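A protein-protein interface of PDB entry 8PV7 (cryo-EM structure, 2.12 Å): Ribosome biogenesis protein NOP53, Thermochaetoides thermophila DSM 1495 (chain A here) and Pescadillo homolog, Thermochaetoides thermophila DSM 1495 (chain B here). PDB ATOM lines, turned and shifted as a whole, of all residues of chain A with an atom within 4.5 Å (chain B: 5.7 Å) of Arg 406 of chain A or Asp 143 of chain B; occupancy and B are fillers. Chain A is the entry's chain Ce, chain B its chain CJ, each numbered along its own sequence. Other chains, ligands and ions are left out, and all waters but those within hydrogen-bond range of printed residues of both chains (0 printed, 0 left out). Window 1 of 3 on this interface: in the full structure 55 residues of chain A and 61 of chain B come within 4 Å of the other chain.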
ATOM      1  N   ALA A 205      -7.512   2.285 -24.899  1.00  0.00           N
ATOM      2  CA  ALA A 205      -8.403   3.289 -25.469  1.00  0.00           C
ATOM      3  C   ALA A 205      -9.306   2.681 -26.534  1.00  0.00           C
ATOM      4  O   ALA A 205     -10.508   2.959 -26.579  1.00  0.00           O
ATOM      5  CB  ALA A 205      -7.586   4.442 -26.048  1.00  0.00           C
ATOM      6  N   LEU A 402     -20.917   5.458 -31.031  1.00  0.00           N
ATOM      7  CA  LEU A 402     -19.476   5.628 -30.896  1.00  0.00           C
ATOM      8  C   LEU A 402     -19.129   6.806 -29.995  1.00  0.00           C
ATOM      9  O   LEU A 402     -18.140   6.754 -29.259  1.00  0.00           O
ATOM     10  CB  LEU A 402     -18.834   5.778 -32.272  1.00  0.00           C
ATOM     11  CG  LEU A 402     -18.794   4.506 -33.122  1.00  0.00           C
ATOM     12  CD1 LEU A 402     -17.837   4.674 -34.272  1.00  0.00           C
ATOM     13  CD2 LEU A 402     -18.389   3.302 -32.292  1.00  0.00           C
ATOM     14  N   LEU A 403     -19.937   7.869 -30.024  1.00  0.00           N
ATOM     15  CA  LEU A 403     -19.708   9.000 -29.128  1.00  0.00           C
ATOM     16  C   LEU A 403     -19.899   8.596 -27.673  1.00  0.00           C
ATOM     17  O   LEU A 403     -19.092   8.953 -26.802  1.00  0.00           O
ATOM     18  CB  LEU A 403     -20.644  10.148 -29.500  1.00  0.00           C
ATOM     19  CG  LEU A 403     -20.507  11.454 -28.721  1.00  0.00           C
ATOM     20  CD1 LEU A 403     -19.107  12.028 -28.867  1.00  0.00           C
ATOM     21  CD2 LEU A 403     -21.548  12.449 -29.185  1.00  0.00           C
ATOM     22  N   LYS A 404     -20.951   7.821 -27.402  1.00  0.00           N
ATOM     23  CA  LYS A 404     -21.179   7.294 -26.064  1.00  0.00           C
ATOM     24  C   LYS A 404     -20.072   6.333 -25.659  1.00  0.00           C
ATOM     25  O   LYS A 404     -19.678   6.288 -24.489  1.00  0.00           O
ATOM     26  CB  LYS A 404     -22.540   6.608 -26.005  1.00  0.00           C
ATOM     27  CG  LYS A 404     -22.995   6.254 -24.607  1.00  0.00           C
ATOM     28  CD  LYS A 404     -24.395   5.677 -24.617  1.00  0.00           C
ATOM     29  CE  LYS A 404     -24.874   5.382 -23.210  1.00  0.00           C
ATOM     30  NZ  LYS A 404     -26.229   4.769 -23.209  1.00  0.00           N
ATOM     31  N   ASP A 405     -19.550   5.567 -26.621  1.00  0.00           N
ATOM     32  CA  ASP A 405     -18.443   4.659 -26.338  1.00  0.00           C
ATOM     33  C   ASP A 405     -17.183   5.421 -25.947  1.00  0.00           C
ATOM     34  O   ASP A 405     -16.471   5.018 -25.023  1.00  0.00           O
ATOM     35  CB  ASP A 405     -18.178   3.772 -27.550  1.00  0.00           C
ATOM     36  CG  ASP A 405     -18.804   2.406 -27.414  1.00  0.00           C
ATOM     37  OD1 ASP A 405     -18.583   1.755 -26.374  1.00  0.00           O
ATOM     38  OD2 ASP A 405     -19.527   1.986 -28.341  1.00  0.00           O
ATOM     39  N   ARG A 406     -16.894   6.526 -26.637  1.00  0.00           N
ATOM     40  CA  ARG A 406     -15.712   7.316 -26.300  1.00  0.00           C
ATOM     41  C   ARG A 406     -15.862   7.983 -24.938  1.00  0.00           C
ATOM     42  O   ARG A 406     -14.901   8.051 -24.161  1.00  0.00           O
ATOM     43  CB  ARG A 406     -15.438   8.361 -27.382  1.00  0.00           C
ATOM     44  CG  ARG A 406     -15.167   7.787 -28.755  1.00  0.00           C
ATOM     45  CD  ARG A 406     -13.691   7.717 -29.110  1.00  0.00           C
ATOM     46  NE  ARG A 406     -12.880   7.113 -28.060  1.00  0.00           N
ATOM     47  CZ  ARG A 406     -12.786   5.811 -27.835  1.00  0.00           C
ATOM     48  NH1 ARG A 406     -13.476   4.936 -28.544  1.00  0.00           N
ATOM     49  NH2 ARG A 406     -11.976   5.377 -26.878  1.00  0.00           N
ATOM     50  N   TYR A 407     -17.068   8.467 -24.626  1.00  0.00           N
ATOM     51  CA  TYR A 407     -17.322   9.042 -23.305  1.00  0.00           C
ATOM     52  C   TYR A 407     -17.180   7.998 -22.195  1.00  0.00           C
ATOM     53  O   TYR A 407     -16.564   8.265 -21.149  1.00  0.00           O
ATOM     54  CB  TYR A 407     -18.711   9.676 -23.294  1.00  0.00           C
ATOM     55  CG  TYR A 407     -19.078  10.362 -22.005  1.00  0.00           C
ATOM     56  CD1 TYR A 407     -18.325  11.417 -21.516  1.00  0.00           C
ATOM     57  CD2 TYR A 407     -20.188   9.957 -21.278  1.00  0.00           C
ATOM     58  CE1 TYR A 407     -18.663  12.043 -20.338  1.00  0.00           C
ATOM     59  CE2 TYR A 407     -20.537  10.579 -20.105  1.00  0.00           C
ATOM     60  CZ  TYR A 407     -19.772  11.620 -19.637  1.00  0.00           C
ATOM     61  OH  TYR A 407     -20.115  12.237 -18.460  1.00  0.00           O
ATOM     62  N   ARG A 408     -17.722   6.795 -22.414  1.00  0.00           N
ATOM     63  CA  ARG A 408     -17.573   5.719 -21.441  1.00  0.00           C
ATOM     64  C   ARG A 408     -16.118   5.318 -21.281  1.00  0.00           C
ATOM     65  O   ARG A 408     -15.680   4.993 -20.175  1.00  0.00           O
ATOM     66  CB  ARG A 408     -18.395   4.500 -21.847  1.00  0.00           C
ATOM     67  CG  ARG A 408     -19.854   4.539 -21.480  1.00  0.00           C
ATOM     68  CD  ARG A 408     -20.475   3.173 -21.729  1.00  0.00           C
ATOM     69  NE  ARG A 408     -19.750   2.109 -21.042  1.00  0.00           N
ATOM     70  CZ  ARG A 408     -20.156   1.534 -19.920  1.00  0.00           C
ATOM     71  NH1 ARG A 408     -21.303   1.863 -19.350  1.00  0.00           N
ATOM     72  NH2 ARG A 408     -19.398   0.596 -19.359  1.00  0.00           N
ATOM     73  N   SER A 409     -15.364   5.311 -22.382  1.00  0.00           N
ATOM     74  CA  SER A 409     -13.949   4.972 -22.319  1.00  0.00           C
ATOM     75  C   SER A 409     -13.180   5.994 -21.497  1.00  0.00           C
ATOM     76  O   SER A 409     -12.297   5.629 -20.712  1.00  0.00           O
ATOM     77  CB  SER A 409     -13.380   4.867 -23.732  1.00  0.00           C
ATOM     78  OG  SER A 409     -12.010   4.524 -23.709  1.00  0.00           O
ATOM     79  N   MET A 410     -13.520   7.278 -21.654  1.00  0.00           N
ATOM     80  CA  MET A 410     -12.896   8.327 -20.853  1.00  0.00           C
ATOM     81  C   MET A 410     -13.161   8.115 -19.367  1.00  0.00           C
ATOM     82  O   MET A 410     -12.239   8.192 -18.542  1.00  0.00           O
ATOM     83  CB  MET A 410     -13.425   9.692 -21.283  1.00  0.00           C
ATOM     84  CG  MET A 410     -12.850  10.210 -22.576  1.00  0.00           C
ATOM     85  SD  MET A 410     -11.074  10.003 -22.709  1.00  0.00           S
ATOM     86  CE  MET A 410     -10.831  10.479 -24.411  1.00  0.00           C
ATOM     87  N   ARG A 413     -11.349   4.776 -18.059  1.00  0.00           N
ATOM     88  CA  ARG A 413      -9.920   4.980 -17.897  1.00  0.00           C
ATOM     89  C   ARG A 413      -9.590   6.093 -16.917  1.00  0.00           C
ATOM     90  O   ARG A 413      -8.415   6.288 -16.600  1.00  0.00           O
ATOM     91  CB  ARG A 413      -9.270   5.258 -19.245  1.00  0.00           C
ATOM     92  CG  ARG A 413      -9.184   4.027 -20.113  1.00  0.00           C
ATOM     93  CD  ARG A 413      -8.546   4.363 -21.421  1.00  0.00           C
ATOM     94  NE  ARG A 413      -9.428   5.199 -22.215  1.00  0.00           N
ATOM     95  CZ  ARG A 413      -9.012   6.185 -22.993  1.00  0.00           C
ATOM     96  NH1 ARG A 413      -7.729   6.483 -23.100  1.00  0.00           N
ATOM     97  NH2 ARG A 413      -9.907   6.896 -23.670  1.00  0.00           N
ATOM     98  N   LYS A 415     -10.001   9.529 -16.802  1.00  0.00           N
ATOM     99  CA  LYS A 415      -9.631  10.902 -17.099  1.00  0.00           C
ATOM    100  C   LYS A 415     -10.661  11.892 -16.575  1.00  0.00           C
ATOM    101  O   LYS A 415     -10.331  13.060 -16.353  1.00  0.00           O
ATOM    102  CB  LYS A 415      -9.432  11.064 -18.603  1.00  0.00           C
ATOM    103  CG  LYS A 415      -8.354  10.156 -19.143  1.00  0.00           C
ATOM    104  CD  LYS A 415      -8.154  10.341 -20.628  1.00  0.00           C
ATOM    105  CE  LYS A 415      -7.028   9.463 -21.132  1.00  0.00           C
ATOM    106  NZ  LYS A 415      -6.833   9.612 -22.596  1.00  0.00           N
ATOM    107  N   ASP B 140      -0.651   7.688 -28.004  1.00  0.00           N
ATOM    108  CA  ASP B 140      -1.972   8.275 -27.768  1.00  0.00           C
ATOM    109  C   ASP B 140      -2.766   8.511 -29.055  1.00  0.00           C
ATOM    110  O   ASP B 140      -3.936   8.948 -29.004  1.00  0.00           O
ATOM    111  CB  ASP B 140      -1.847   9.578 -26.983  1.00  0.00           C
ATOM    112  CG  ASP B 140      -2.923   9.717 -25.932  1.00  0.00           C
ATOM    113  OD1 ASP B 140      -3.240   8.704 -25.279  1.00  0.00           O
ATOM    114  OD2 ASP B 140      -3.459  10.830 -25.764  1.00  0.00           O
ATOM    115  N   LEU B 141      -2.150   8.239 -30.210  1.00  0.00           N
ATOM    116  CA  LEU B 141      -2.846   8.399 -31.483  1.00  0.00           C
ATOM    117  C   LEU B 141      -4.114   7.560 -31.617  1.00  0.00           C
ATOM    118  O   LEU B 141      -4.978   7.938 -32.403  1.00  0.00           O
ATOM    119  CB  LEU B 141      -1.921   8.069 -32.651  1.00  0.00           C
ATOM    120  CG  LEU B 141      -1.230   9.261 -33.301  1.00  0.00           C
ATOM    121  CD1 LEU B 141      -0.532   8.815 -34.563  1.00  0.00           C
ATOM    122  CD2 LEU B 141      -2.223  10.366 -33.601  1.00  0.00           C
ATOM    123  N   ASP B 142      -4.260   6.454 -30.884  1.00  0.00           N
ATOM    124  CA  ASP B 142      -5.472   5.642 -31.009  1.00  0.00           C
ATOM    125  C   ASP B 142      -6.707   6.420 -30.568  1.00  0.00           C
ATOM    126  O   ASP B 142      -7.690   6.538 -31.318  1.00  0.00           O
ATOM    127  CB  ASP B 142      -5.337   4.361 -30.189  1.00  0.00           C
ATOM    128  CG  ASP B 142      -4.220   3.470 -30.679  1.00  0.00           C
ATOM    129  OD1 ASP B 142      -3.330   3.968 -31.399  1.00  0.00           O
ATOM    130  OD2 ASP B 142      -4.226   2.269 -30.341  1.00  0.00           O
ATOM    131  N   ASP B 143      -6.652   6.990 -29.362  1.00  0.00           N
ATOM    132  CA  ASP B 143      -7.733   7.831 -28.869  1.00  0.00           C
ATOM    133  C   ASP B 143      -7.903   9.076 -29.727  1.00  0.00           C
ATOM    134  O   ASP B 143      -9.038   9.466 -30.043  1.00  0.00           O
ATOM    135  CB  ASP B 143      -7.468   8.226 -27.419  1.00  0.00           C
ATOM    136  CG  ASP B 143      -8.737   8.419 -26.637  1.00  0.00           C
ATOM    137  OD1 ASP B 143      -9.651   9.103 -27.139  1.00  0.00           O
ATOM    138  OD2 ASP B 143      -8.823   7.893 -25.516  1.00  0.00           O
ATOM    139  N   CYS B 144      -6.783   9.703 -30.119  1.00  0.00           N
ATOM    140  CA  CYS B 144      -6.866  10.912 -30.939  1.00  0.00           C
ATOM    141  C   CYS B 144      -7.590  10.654 -32.261  1.00  0.00           C
ATOM    142  O   CYS B 144      -8.506  11.397 -32.639  1.00  0.00           O
ATOM    143  CB  CYS B 144      -5.464  11.464 -31.199  1.00  0.00           C
ATOM    144  SG  CYS B 144      -5.405  12.915 -32.266  1.00  0.00           S
ATOM    145  N   LEU B 145      -7.217   9.576 -32.954  1.00  0.00           N
ATOM    146  CA  LEU B 145      -7.780   9.295 -34.266  1.00  0.00           C
ATOM    147  C   LEU B 145      -9.227   8.846 -34.170  1.00  0.00           C
ATOM    148  O   LEU B 145     -10.044   9.228 -35.013  1.00  0.00           O
ATOM    149  CB  LEU B 145      -6.951   8.241 -34.988  1.00  0.00           C
ATOM    150  CG  LEU B 145      -5.578   8.677 -35.485  1.00  0.00           C
ATOM    151  CD1 LEU B 145      -4.817   7.449 -35.933  1.00  0.00           C
ATOM    152  CD2 LEU B 145      -5.672   9.715 -36.582  1.00  0.00           C
ATOM    153  N   SER B 146      -9.568   8.039 -33.156  1.00  0.00           N
ATOM    154  CA  SER B 146     -10.965   7.653 -32.986  1.00  0.00           C
ATOM    155  C   SER B 146     -11.850   8.870 -32.753  1.00  0.00           C
ATOM    156  O   SER B 146     -12.886   9.023 -33.416  1.00  0.00           O
ATOM    157  CB  SER B 146     -11.115   6.656 -31.842  1.00  0.00           C
ATOM    158  OG  SER B 146     -10.531   5.416 -32.178  1.00  0.00           O
ATOM    159  N   MET B 147     -11.413   9.789 -31.883  1.00  0.00           N
ATOM    160  CA  MET B 147     -12.221  10.969 -31.593  1.00  0.00           C
ATOM    161  C   MET B 147     -12.349  11.877 -32.815  1.00  0.00           C
ATOM    162  O   MET B 147     -13.442  12.369 -33.119  1.00  0.00           O
ATOM    163  CB  MET B 147     -11.624  11.731 -30.410  1.00  0.00           C
ATOM    164  CG  MET B 147     -11.946  11.102 -29.062  1.00  0.00           C
ATOM    165  SD  MET B 147     -13.457  11.654 -28.255  1.00  0.00           S
ATOM    166  CE  MET B 147     -13.525  13.353 -28.774  1.00  0.00           C
ATOM    167  N   LEU B 148     -11.252  12.090 -33.548  1.00  0.00           N
ATOM    168  CA  LEU B 148     -11.312  13.043 -34.653  1.00  0.00           C
ATOM    169  C   LEU B 148     -12.056  12.474 -35.857  1.00  0.00           C
ATOM    170  O   LEU B 148     -12.819  13.198 -36.513  1.00  0.00           O
ATOM    171  CB  LEU B 148      -9.910  13.506 -35.036  1.00  0.00           C
ATOM    172  CG  LEU B 148      -9.271  14.424 -33.990  1.00  0.00           C
ATOM    173  CD1 LEU B 148      -7.962  14.984 -34.485  1.00  0.00           C
ATOM    174  CD2 LEU B 148     -10.218  15.543 -33.593  1.00  0.00           C
ATOM    175  N   LEU B 150     -14.448  10.355 -35.611  1.00  0.00           N
ATOM    176  CA  LEU B 150     -15.848  10.430 -35.221  1.00  0.00           C
ATOM    177  C   LEU B 150     -16.407  11.834 -35.423  1.00  0.00           C
ATOM    178  O   LEU B 150     -17.487  12.004 -35.997  1.00  0.00           O
ATOM    179  CB  LEU B 150     -15.994   9.997 -33.770  1.00  0.00           C
ATOM    180  CG  LEU B 150     -17.357  10.146 -33.115  1.00  0.00           C
ATOM    181  CD1 LEU B 150     -18.434   9.414 -33.894  1.00  0.00           C
ATOM    182  CD2 LEU B 150     -17.245   9.610 -31.721  1.00  0.00           C
ATOM    183  N   LEU B 207      -4.300   1.459 -33.667  1.00  0.00           N
ATOM    184  CA  LEU B 207      -5.616   0.915 -33.970  1.00  0.00           C
ATOM    185  C   LEU B 207      -6.674   1.961 -33.659  1.00  0.00           C
ATOM    186  O   LEU B 207      -6.707   2.497 -32.547  1.00  0.00           O
ATOM    187  CB  LEU B 207      -5.876  -0.349 -33.154  1.00  0.00           C
ATOM    188  CG  LEU B 207      -7.280  -0.935 -33.223  1.00  0.00           C
ATOM    189  CD1 LEU B 207      -7.469  -1.701 -34.515  1.00  0.00           C
ATOM    190  CD2 LEU B 207      -7.545  -1.814 -32.016  1.00  0.00           C
ATOM    191  N   LEU B 209     -10.996   3.312 -34.576  1.00  0.00           N
ATOM    192  CA  LEU B 209     -12.334   2.932 -35.002  1.00  0.00           C
ATOM    193  C   LEU B 209     -13.020   4.117 -35.666  1.00  0.00           C
ATOM    194  O   LEU B 209     -13.060   5.212 -35.100  1.00  0.00           O
ATOM    195  CB  LEU B 209     -13.147   2.444 -33.804  1.00  0.00           C
ATOM    196  CG  LEU B 209     -14.582   1.982 -34.017  1.00  0.00           C
ATOM    197  CD1 LEU B 209     -14.659   0.934 -35.109  1.00  0.00           C
ATOM    198  CD2 LEU B 209     -15.127   1.445 -32.709  1.00  0.00           C
ATOM    199  N   MET B 227     -16.500  16.711 -24.471  1.00  0.00           N
ATOM    200  CA  MET B 227     -16.000  16.008 -25.648  1.00  0.00           C
ATOM    201  C   MET B 227     -15.412  16.984 -26.661  1.00  0.00           C
ATOM    202  O   MET B 227     -14.409  16.683 -27.315  1.00  0.00           O
ATOM    203  CB  MET B 227     -17.106  15.172 -26.287  1.00  0.00           C
ATOM    204  CG  MET B 227     -17.590  14.033 -25.419  1.00  0.00           C
ATOM    205  SD  MET B 227     -16.250  12.996 -24.818  1.00  0.00           S
ATOM    206  CE  MET B 227     -16.411  11.599 -25.914  1.00  0.00           C
ATOM    207  N   TYR B 234      -7.078  17.223 -29.247  1.00  0.00           N
ATOM    208  CA  TYR B 234      -6.608  16.200 -30.172  1.00  0.00           C
ATOM    209  C   TYR B 234      -6.326  16.754 -31.559  1.00  0.00           C
ATOM    210  O   TYR B 234      -5.426  16.254 -32.232  1.00  0.00           O
ATOM    211  CB  TYR B 234      -7.603  15.047 -30.246  1.00  0.00           C
ATOM    212  CG  TYR B 234      -7.458  14.104 -29.087  1.00  0.00           C
ATOM    213  CD1 TYR B 234      -6.202  13.788 -28.590  1.00  0.00           C
ATOM    214  CD2 TYR B 234      -8.565  13.536 -28.481  1.00  0.00           C
ATOM    215  CE1 TYR B 234      -6.052  12.933 -27.527  1.00  0.00           C
ATOM    216  CE2 TYR B 234      -8.424  12.678 -27.415  1.00  0.00           C
ATOM    217  CZ  TYR B 234      -7.164  12.381 -26.944  1.00  0.00           C
ATOM    218  OH  TYR B 234      -7.016  11.527 -25.883  1.00  0.00           O
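The guanidinium group of Arg 413 of chain A lies within salt-bridge range of the side-chain carboxylate of Asp 143 of chain B (3.0 Å). The side-chain amino group (NZ) of Lys 415 of chain A is in salt-bridge range of the side-chain carboxylate (OD2) of Asp 143 of chain B (3.9 Å). The guanidinium group of Arg 406 of chain A lies within salt-bridge range of the side-chain carboxylate of Asp 143 of chain B.
The backbone NH of Leu 209 of chain B is in hydrogen-bond range of the side-chain hydroxyl of Ser 146 of chain B (3.2 Å). The side-chain hydroxyl (OG) of Ser 146 of chain B sits at hydrogen-bond distance from the backbone carbonyl oxygen (O) of Asp 142 of chain B (3.2 Å). The backbone carbonyl oxygen of Ala 205 of chain A lies within hydrogen-bond range of the guanidinium group of Arg 406 of chain A (2.8 Å). NE of Arg 413 of chain A lies within hydrogen-bond range of OG of Ser 409 of chain A (3.1 Å). The side-chain sulfur (SG) of Cys 144 of chain B lies within hydrogen-bond range of the backbone carbonyl oxygen (O) of Tyr 234 of chain B (3.3 Å). The guanidinium group of Arg 413 of chain A sits at hydrogen-bond distance from the side-chain sulfur of Met 410 of chain A (3.5 Å).
Among the printed residues, merely in contact across the chains: Met 410 of chain A with Asp 143 of chain B, Tyr 407 of chain A with Met 227 of chain B, Leu 403 of chain A with Leu 150 of chain B, Arg 406 of chain A with Met 227 of chain B, Ala 205 of chain A with Asp 143 of chain B, Leu 402 of chain A with Leu 209 of chain B, Leu 402 of chain A with Leu 150 of chain B, Lys 415 of chain A with Tyr 234 of chain B, Arg 406 of chain A with Met 147 of chain B, Leu 403 of chain A with Met 227 of chain B and Arg 406 of chain A with Ser 146 of chain B.
Of the printed residues of chain B, Ala 205 of chain A touches Asp 143. Arg 406 of chain A touches four residues of chain B. Ser 409 of chain A touches none of the printed residues of chain B. Of the printed residues of chain B, Arg 413 of chain A touches Asp 143 (2.4 Å). Asp 143 of chain B touches five residues of chain A. Cys 144 of chain B touches none of the printed residues of chain A. Of the printed residues of chain A, Met 147 of chain B touches Arg 406. Printed residues of chain A within 4 Å of Tyr 234 of chain B: Lys 415 (3.8 Å). The nearest printed residue of chain A that does not touch Asp 143 of chain B is Ser 409 of chain A (5.0 Å). The nearest printed residue of chain B that does not touch Arg 413 of chain A is Asp 140 of chain B (5.5 Å).
Of the 12 printed residues of chain A, 8 touch a printed residue of chain B. Hydrophobic or aromatic side chains of chain A within 4 Å of the printed part of chain B: Ala 205, Leu 402, Tyr 407 and Met 410. Along chain A the printed residues that touch a printed residue of chain B span positions 205 to 415. Among the printed residues, 14 pairs touch across the chains.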
